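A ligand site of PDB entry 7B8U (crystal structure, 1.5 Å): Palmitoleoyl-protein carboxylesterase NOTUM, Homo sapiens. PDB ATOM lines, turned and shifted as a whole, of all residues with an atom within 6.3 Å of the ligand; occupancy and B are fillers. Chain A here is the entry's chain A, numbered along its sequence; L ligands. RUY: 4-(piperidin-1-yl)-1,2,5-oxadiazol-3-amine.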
ATOM      1  N   GLY A  50     -30.858 -12.755  16.159  1.00  0.00           N
ATOM      2  CA  GLY A  50     -29.767 -11.792  16.320  1.00  0.00           C
ATOM      3  C   GLY A  50     -28.593 -12.194  17.202  1.00  0.00           C
ATOM      4  O   GLY A  50     -28.185 -11.404  18.073  1.00  0.00           O
ATOM      5  N   TRP A  51     -28.020 -13.371  16.981  1.00  0.00           N
ATOM      6  CA  TRP A  51     -26.836 -13.892  17.715  1.00  0.00           C
ATOM      7  C   TRP A  51     -27.145 -13.948  19.221  1.00  0.00           C
ATOM      8  O   TRP A  51     -28.268 -14.310  19.589  1.00  0.00           O
ATOM      9  CB  TRP A  51     -25.587 -13.116  17.321  1.00  0.00           C
ATOM     10  CG  TRP A  51     -25.183 -13.436  15.894  1.00  0.00           C
ATOM     11  CD1 TRP A  51     -25.440 -12.689  14.781  1.00  0.00           C
ATOM     12  CD2 TRP A  51     -24.520 -14.625  15.432  1.00  0.00           C
ATOM     13  NE1 TRP A  51     -24.926 -13.322  13.662  1.00  0.00           N
ATOM     14  CE2 TRP A  51     -24.379 -14.505  14.035  1.00  0.00           C
ATOM     15  CE3 TRP A  51     -24.020 -15.759  16.075  1.00  0.00           C
ATOM     16  CZ2 TRP A  51     -23.756 -15.497  13.265  1.00  0.00           C
ATOM     17  CZ3 TRP A  51     -23.397 -16.751  15.305  1.00  0.00           C
ATOM     18  CH2 TRP A  51     -23.282 -16.604  13.911  1.00  0.00           C
ATOM     19  N   TYR A  52     -26.152 -13.700  20.085  1.00  0.00           N
ATOM     20  CA  TYR A  52     -26.273 -13.847  21.535  1.00  0.00           C
ATOM     21  C   TYR A  52     -25.018 -13.228  22.147  1.00  0.00           C
ATOM     22  O   TYR A  52     -24.092 -12.841  21.430  1.00  0.00           O
ATOM     23  CB  TYR A  52     -26.403 -15.311  21.973  1.00  0.00           C
ATOM     24  CG  TYR A  52     -25.331 -16.218  21.414  1.00  0.00           C
ATOM     25  CD1 TYR A  52     -25.514 -16.910  20.213  1.00  0.00           C
ATOM     26  CD2 TYR A  52     -24.142 -16.415  22.098  1.00  0.00           C
ATOM     27  CE1 TYR A  52     -24.529 -17.747  19.711  1.00  0.00           C
ATOM     28  CE2 TYR A  52     -23.152 -17.242  21.605  1.00  0.00           C
ATOM     29  CZ  TYR A  52     -23.352 -17.910  20.417  1.00  0.00           C
ATOM     30  OH  TYR A  52     -22.348 -18.736  19.950  1.00  0.00           O
ATOM     31  N   TYR A 105     -36.484  -9.794  20.207  1.00  0.00           N
ATOM     32  CA  TYR A 105     -35.416 -10.531  20.878  1.00  0.00           C
ATOM     33  C   TYR A 105     -34.581  -9.520  21.659  1.00  0.00           C
ATOM     34  O   TYR A 105     -33.776  -8.794  21.087  1.00  0.00           O
ATOM     35  CB  TYR A 105     -34.599 -11.274  19.821  1.00  0.00           C
ATOM     36  CG  TYR A 105     -33.426 -12.117  20.282  1.00  0.00           C
ATOM     37  CD1 TYR A 105     -33.510 -12.951  21.403  1.00  0.00           C
ATOM     38  CD2 TYR A 105     -32.249 -12.145  19.534  1.00  0.00           C
ATOM     39  CE1 TYR A 105     -32.421 -13.767  21.794  1.00  0.00           C
ATOM     40  CE2 TYR A 105     -31.176 -12.962  19.899  1.00  0.00           C
ATOM     41  CZ  TYR A 105     -31.263 -13.766  21.022  1.00  0.00           C
ATOM     42  OH  TYR A 105     -30.189 -14.559  21.381  1.00  0.00           O
ATOM     43  N   VAL A 110     -30.622 -16.904  23.092  1.00  0.00           N
ATOM     44  CA  VAL A 110     -31.193 -17.840  22.122  1.00  0.00           C
ATOM     45  C   VAL A 110     -32.562 -18.307  22.674  1.00  0.00           C
ATOM     46  O   VAL A 110     -33.013 -19.447  22.486  1.00  0.00           O
ATOM     47  CB  VAL A 110     -30.222 -19.014  21.843  1.00  0.00           C
ATOM     48  CG1 VAL A 110     -30.765 -20.025  20.822  1.00  0.00           C
ATOM     49  CG2 VAL A 110     -28.789 -18.546  21.535  1.00  0.00           C
ATOM     50  N   SER A 155     -33.328 -17.784  12.594  1.00  0.00           N
ATOM     51  CA  SER A 155     -31.930 -17.831  13.103  1.00  0.00           C
ATOM     52  C   SER A 155     -31.966 -18.125  14.592  1.00  0.00           C
ATOM     53  O   SER A 155     -32.457 -19.201  14.972  1.00  0.00           O
ATOM     54  CB  SER A 155     -31.156 -16.579  12.688  1.00  0.00           C
ATOM     55  OG  SER A 155     -29.766 -16.860  12.727  1.00  0.00           O
ATOM     56  N   ALA A 156     -31.454 -17.252  15.483  1.00  0.00           N
ATOM     57  CA  ALA A 156     -31.557 -17.540  16.918  1.00  0.00           C
ATOM     58  C   ALA A 156     -33.016 -17.765  17.329  1.00  0.00           C
ATOM     59  O   ALA A 156     -33.293 -18.519  18.268  1.00  0.00           O
ATOM     60  CB  ALA A 156     -30.945 -16.423  17.761  1.00  0.00           C
ATOM     61  N   GLY A 157     -33.957 -17.124  16.624  1.00  0.00           N
ATOM     62  CA  GLY A 157     -35.362 -17.375  16.900  1.00  0.00           C
ATOM     63  C   GLY A 157     -35.831 -18.732  16.403  1.00  0.00           C
ATOM     64  O   GLY A 157     -36.779 -19.307  16.965  1.00  0.00           O
ATOM     65  N   THR A 159     -33.860 -21.500  16.444  1.00  0.00           N
ATOM     66  CA  THR A 159     -33.442 -22.390  17.528  1.00  0.00           C
ATOM     67  C   THR A 159     -34.382 -22.229  18.730  1.00  0.00           C
ATOM     68  O   THR A 159     -34.737 -23.213  19.387  1.00  0.00           O
ATOM     69  CB  THR A 159     -31.985 -22.113  17.920  1.00  0.00           C
ATOM     70  OG1 THR A 159     -31.136 -22.182  16.754  1.00  0.00           O
ATOM     71  CG2 THR A 159     -31.485 -23.155  18.909  1.00  0.00           C
ATOM     72  N   SER A 188     -33.935 -21.355   9.615  1.00  0.00           N
ATOM     73  CA  SER A 188     -32.507 -21.032   9.718  1.00  0.00           C
ATOM     74  C   SER A 188     -31.963 -21.195  11.141  1.00  0.00           C
ATOM     75  O   SER A 188     -31.017 -20.498  11.534  1.00  0.00           O
ATOM     76  CB  SER A 188     -32.239 -19.614   9.209  1.00  0.00           C
ATOM     77  OG  SER A 188     -32.579 -19.539   7.831  1.00  0.00           O
ATOM     78  N   GLY A 189     -32.511 -22.135  11.906  1.00  0.00           N
ATOM     79  CA  GLY A 189     -31.983 -22.395  13.235  1.00  0.00           C
ATOM     80  C   GLY A 189     -31.521 -23.830  13.461  1.00  0.00           C
ATOM     81  O   GLY A 189     -31.435 -24.281  14.616  1.00  0.00           O
ATOM     82  N   PHE A 191     -28.465 -26.048  12.988  1.00  0.00           N
ATOM     83  CA  PHE A 191     -27.017 -26.001  12.829  1.00  0.00           C
ATOM     84  C   PHE A 191     -26.342 -27.338  13.111  1.00  0.00           C
ATOM     85  O   PHE A 191     -26.863 -28.204  13.817  1.00  0.00           O
ATOM     86  CB  PHE A 191     -26.406 -24.914  13.727  1.00  0.00           C
ATOM     87  CG  PHE A 191     -26.954 -23.529  13.482  1.00  0.00           C
ATOM     88  CD1 PHE A 191     -28.025 -23.033  14.218  1.00  0.00           C
ATOM     89  CD2 PHE A 191     -26.421 -22.723  12.489  1.00  0.00           C
ATOM     90  CE1 PHE A 191     -28.527 -21.751  13.990  1.00  0.00           C
ATOM     91  CE2 PHE A 191     -26.935 -21.455  12.249  1.00  0.00           C
ATOM     92  CZ  PHE A 191     -27.985 -20.971  13.011  1.00  0.00           C
ATOM     93  N   LEU A 192     -25.125 -27.473  12.562  1.00  0.00           N
ATOM     94  CA  LEU A 192     -24.261 -28.643  12.747  1.00  0.00           C
ATOM     95  C   LEU A 192     -23.079 -28.277  13.633  1.00  0.00           C
ATOM     96  O   LEU A 192     -22.436 -27.238  13.428  1.00  0.00           O
ATOM     97  CB  LEU A 192     -23.743 -29.171  11.404  1.00  0.00           C
ATOM     98  CG  LEU A 192     -24.768 -29.554  10.330  1.00  0.00           C
ATOM     99  CD1 LEU A 192     -24.029 -30.110   9.144  1.00  0.00           C
ATOM    100  CD2 LEU A 192     -25.761 -30.576  10.900  1.00  0.00           C
ATOM    101  N   PRO A 210     -19.125 -22.573  18.416  1.00  0.00           N
ATOM    102  CA  PRO A 210     -20.506 -22.527  18.966  1.00  0.00           C
ATOM    103  C   PRO A 210     -20.698 -23.426  20.170  1.00  0.00           C
ATOM    104  O   PRO A 210     -21.290 -22.985  21.171  1.00  0.00           O
ATOM    105  CB  PRO A 210     -21.383 -22.958  17.786  1.00  0.00           C
ATOM    106  CG  PRO A 210     -20.519 -22.904  16.599  1.00  0.00           C
ATOM    107  CD  PRO A 210     -19.083 -22.858  16.980  1.00  0.00           C
ATOM    108  N   THR A 211     -20.188 -24.658  20.134  1.00  0.00           N
ATOM    109  CA  THR A 211     -20.428 -25.585  21.236  1.00  0.00           C
ATOM    110  C   THR A 211     -19.836 -25.059  22.548  1.00  0.00           C
ATOM    111  O   THR A 211     -20.455 -25.204  23.615  1.00  0.00           O
ATOM    112  CB  THR A 211     -19.860 -26.973  20.922  1.00  0.00           C
ATOM    113  OG1 THR A 211     -18.451 -26.876  20.692  1.00  0.00           O
ATOM    114  CG2 THR A 211     -20.540 -27.555  19.684  1.00  0.00           C
ATOM    115  N   ILE A 214     -21.840 -21.792  23.671  1.00  0.00           N
ATOM    116  CA  ILE A 214     -23.156 -22.155  24.187  1.00  0.00           C
ATOM    117  C   ILE A 214     -23.042 -22.797  25.559  1.00  0.00           C
ATOM    118  O   ILE A 214     -23.855 -22.539  26.450  1.00  0.00           O
ATOM    119  CB  ILE A 214     -23.896 -23.064  23.191  1.00  0.00           C
ATOM    120  CG1 ILE A 214     -24.272 -22.271  21.934  1.00  0.00           C
ATOM    121  CG2 ILE A 214     -25.157 -23.626  23.813  1.00  0.00           C
ATOM    122  CD1 ILE A 214     -25.007 -23.093  20.895  1.00  0.00           C
ATOM    123  N   PHE A 242     -29.232 -27.497  21.851  1.00  0.00           N
ATOM    124  CA  PHE A 242     -29.274 -26.355  20.945  1.00  0.00           C
ATOM    125  C   PHE A 242     -29.044 -26.745  19.482  1.00  0.00           C
ATOM    126  O   PHE A 242     -29.153 -25.878  18.600  1.00  0.00           O
ATOM    127  CB  PHE A 242     -28.241 -25.284  21.350  1.00  0.00           C
ATOM    128  CG  PHE A 242     -28.618 -24.471  22.563  1.00  0.00           C
ATOM    129  CD1 PHE A 242     -28.715 -23.081  22.463  1.00  0.00           C
ATOM    130  CD2 PHE A 242     -28.827 -25.055  23.799  1.00  0.00           C
ATOM    131  CE1 PHE A 242     -29.050 -22.307  23.560  1.00  0.00           C
ATOM    132  CE2 PHE A 242     -29.169 -24.283  24.922  1.00  0.00           C
ATOM    133  CZ  PHE A 242     -29.261 -22.908  24.793  1.00  0.00           C
ATOM    134  N   PHE A 243     -28.784 -28.015  19.187  1.00  0.00           N
ATOM    135  CA  PHE A 243     -28.523 -28.457  17.823  1.00  0.00           C
ATOM    136  C   PHE A 243     -29.717 -29.255  17.306  1.00  0.00           C
ATOM    137  O   PHE A 243     -30.047 -30.301  17.868  1.00  0.00           O
ATOM    138  CB  PHE A 243     -27.229 -29.269  17.754  1.00  0.00           C
ATOM    139  CG  PHE A 243     -26.009 -28.406  17.961  1.00  0.00           C
ATOM    140  CD1 PHE A 243     -25.643 -28.000  19.226  1.00  0.00           C
ATOM    141  CD2 PHE A 243     -25.363 -27.855  16.864  1.00  0.00           C
ATOM    142  CE1 PHE A 243     -24.571 -27.155  19.416  1.00  0.00           C
ATOM    143  CE2 PHE A 243     -24.284 -26.992  17.042  1.00  0.00           C
ATOM    144  CZ  PHE A 243     -23.898 -26.638  18.323  1.00  0.00           C
ATOM    145  N   ALA A 265     -24.768 -18.175   8.268  1.00  0.00           N
ATOM    146  CA  ALA A 265     -24.343 -18.200   9.665  1.00  0.00           C
ATOM    147  C   ALA A 265     -23.562 -19.468   9.980  1.00  0.00           C
ATOM    148  O   ALA A 265     -22.584 -19.427  10.741  1.00  0.00           O
ATOM    149  CB  ALA A 265     -25.554 -18.071  10.589  1.00  0.00           C
ATOM    150  N   VAL A 269     -19.548 -19.402  11.377  1.00  0.00           N
ATOM    151  CA  VAL A 269     -19.002 -20.085  12.542  1.00  0.00           C
ATOM    152  C   VAL A 269     -18.010 -21.174  12.129  1.00  0.00           C
ATOM    153  O   VAL A 269     -17.198 -21.590  12.967  1.00  0.00           O
ATOM    154  CB  VAL A 269     -20.113 -20.672  13.435  1.00  0.00           C
ATOM    155  CG1 VAL A 269     -21.020 -19.561  13.952  1.00  0.00           C
ATOM    156  CG2 VAL A 269     -20.909 -21.742  12.703  1.00  0.00           C
ATOM    157  N   HIS A 312     -29.441 -16.668   4.225  1.00  0.00           N
ATOM    158  CA  HIS A 312     -29.681 -16.733   5.667  1.00  0.00           C
ATOM    159  C   HIS A 312     -31.029 -16.096   5.971  1.00  0.00           C
ATOM    160  O   HIS A 312     -31.256 -14.936   5.612  1.00  0.00           O
ATOM    161  CB  HIS A 312     -28.566 -16.033   6.455  1.00  0.00           C
ATOM    162  CG  HIS A 312     -28.694 -16.183   7.933  1.00  0.00           C
ATOM    163  ND1 HIS A 312     -28.715 -17.422   8.558  1.00  0.00           N
ATOM    164  CD2 HIS A 312     -28.828 -15.267   8.933  1.00  0.00           C
ATOM    165  CE1 HIS A 312     -28.855 -17.253   9.856  1.00  0.00           C
ATOM    166  NE2 HIS A 312     -28.917 -15.960  10.109  1.00  0.00           N
HETATM  167  N1  RUY L   1     -26.586 -20.513  16.753  1.00  0.00           N
HETATM  168  N3  RUY L   1     -24.905 -22.288  16.610  1.00  0.00           N
HETATM  169  C4  RUY L   1     -25.862 -19.557  15.800  1.00  0.00           C
HETATM  170  C5  RUY L   1     -26.681 -18.310  15.415  1.00  0.00           C
HETATM  171  C6  RUY L   1     -26.114 -21.867  16.930  1.00  0.00           C
HETATM  172  C7  RUY L   1     -26.833 -22.947  17.419  1.00  0.00           C
HETATM  173  C1  RUY L   1     -27.228 -17.637  16.579  1.00  0.00           C
HETATM  174  C2  RUY L   1     -27.999 -18.532  17.430  1.00  0.00           C
HETATM  175  C3  RUY L   1     -27.173 -19.717  17.919  1.00  0.00           C
HETATM  176  N2  RUY L   1     -26.043 -23.994  17.412  1.00  0.00           N
HETATM  177  N4  RUY L   1     -28.210 -22.949  17.878  1.00  0.00           N
HETATM  178  O1  RUY L   1     -24.837 -23.605  16.914  1.00  0.00           O
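N4 of the ligand lies within hydrogen-bond range of OG1 of Thr 159, 3.2 Å away.
A nitrogen (N4) of the ligand lies within hydrogen-bond range of the backbone carbonyl oxygen (O) of Phe 242 (3.2 Å).
The side-chain hydroxyl (OG1) of Thr 159 lies within hydrogen-bond range of the backbone carbonyl oxygen (O) of Gly 189, 3.0 Å away.
O of Trp 51 is in hydrogen-bond range of OH of Tyr 105 (2.6 Å).
Residues that only touch the ligand: Phe 191 (3.4 Å), Phe 243 (3.4 Å), Pro 210 (3.6 Å), Trp 51 (3.6 Å), Ala 156 (3.6 Å), Ile 214 (3.7 Å) and Tyr 52 (3.8 Å).
Hydrophobic or aromatic side chains within 4 Å of the ligand: Trp 51, Tyr 52, Ala 156, Phe 191, Pro 210, Ile 214 and Phe 243.
Within 4 Å of the ligand: Trp 51, Tyr 52, Ala 156, Thr 159, Phe 191, Pro 210, Ile 214, Phe 242 and Phe 243.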
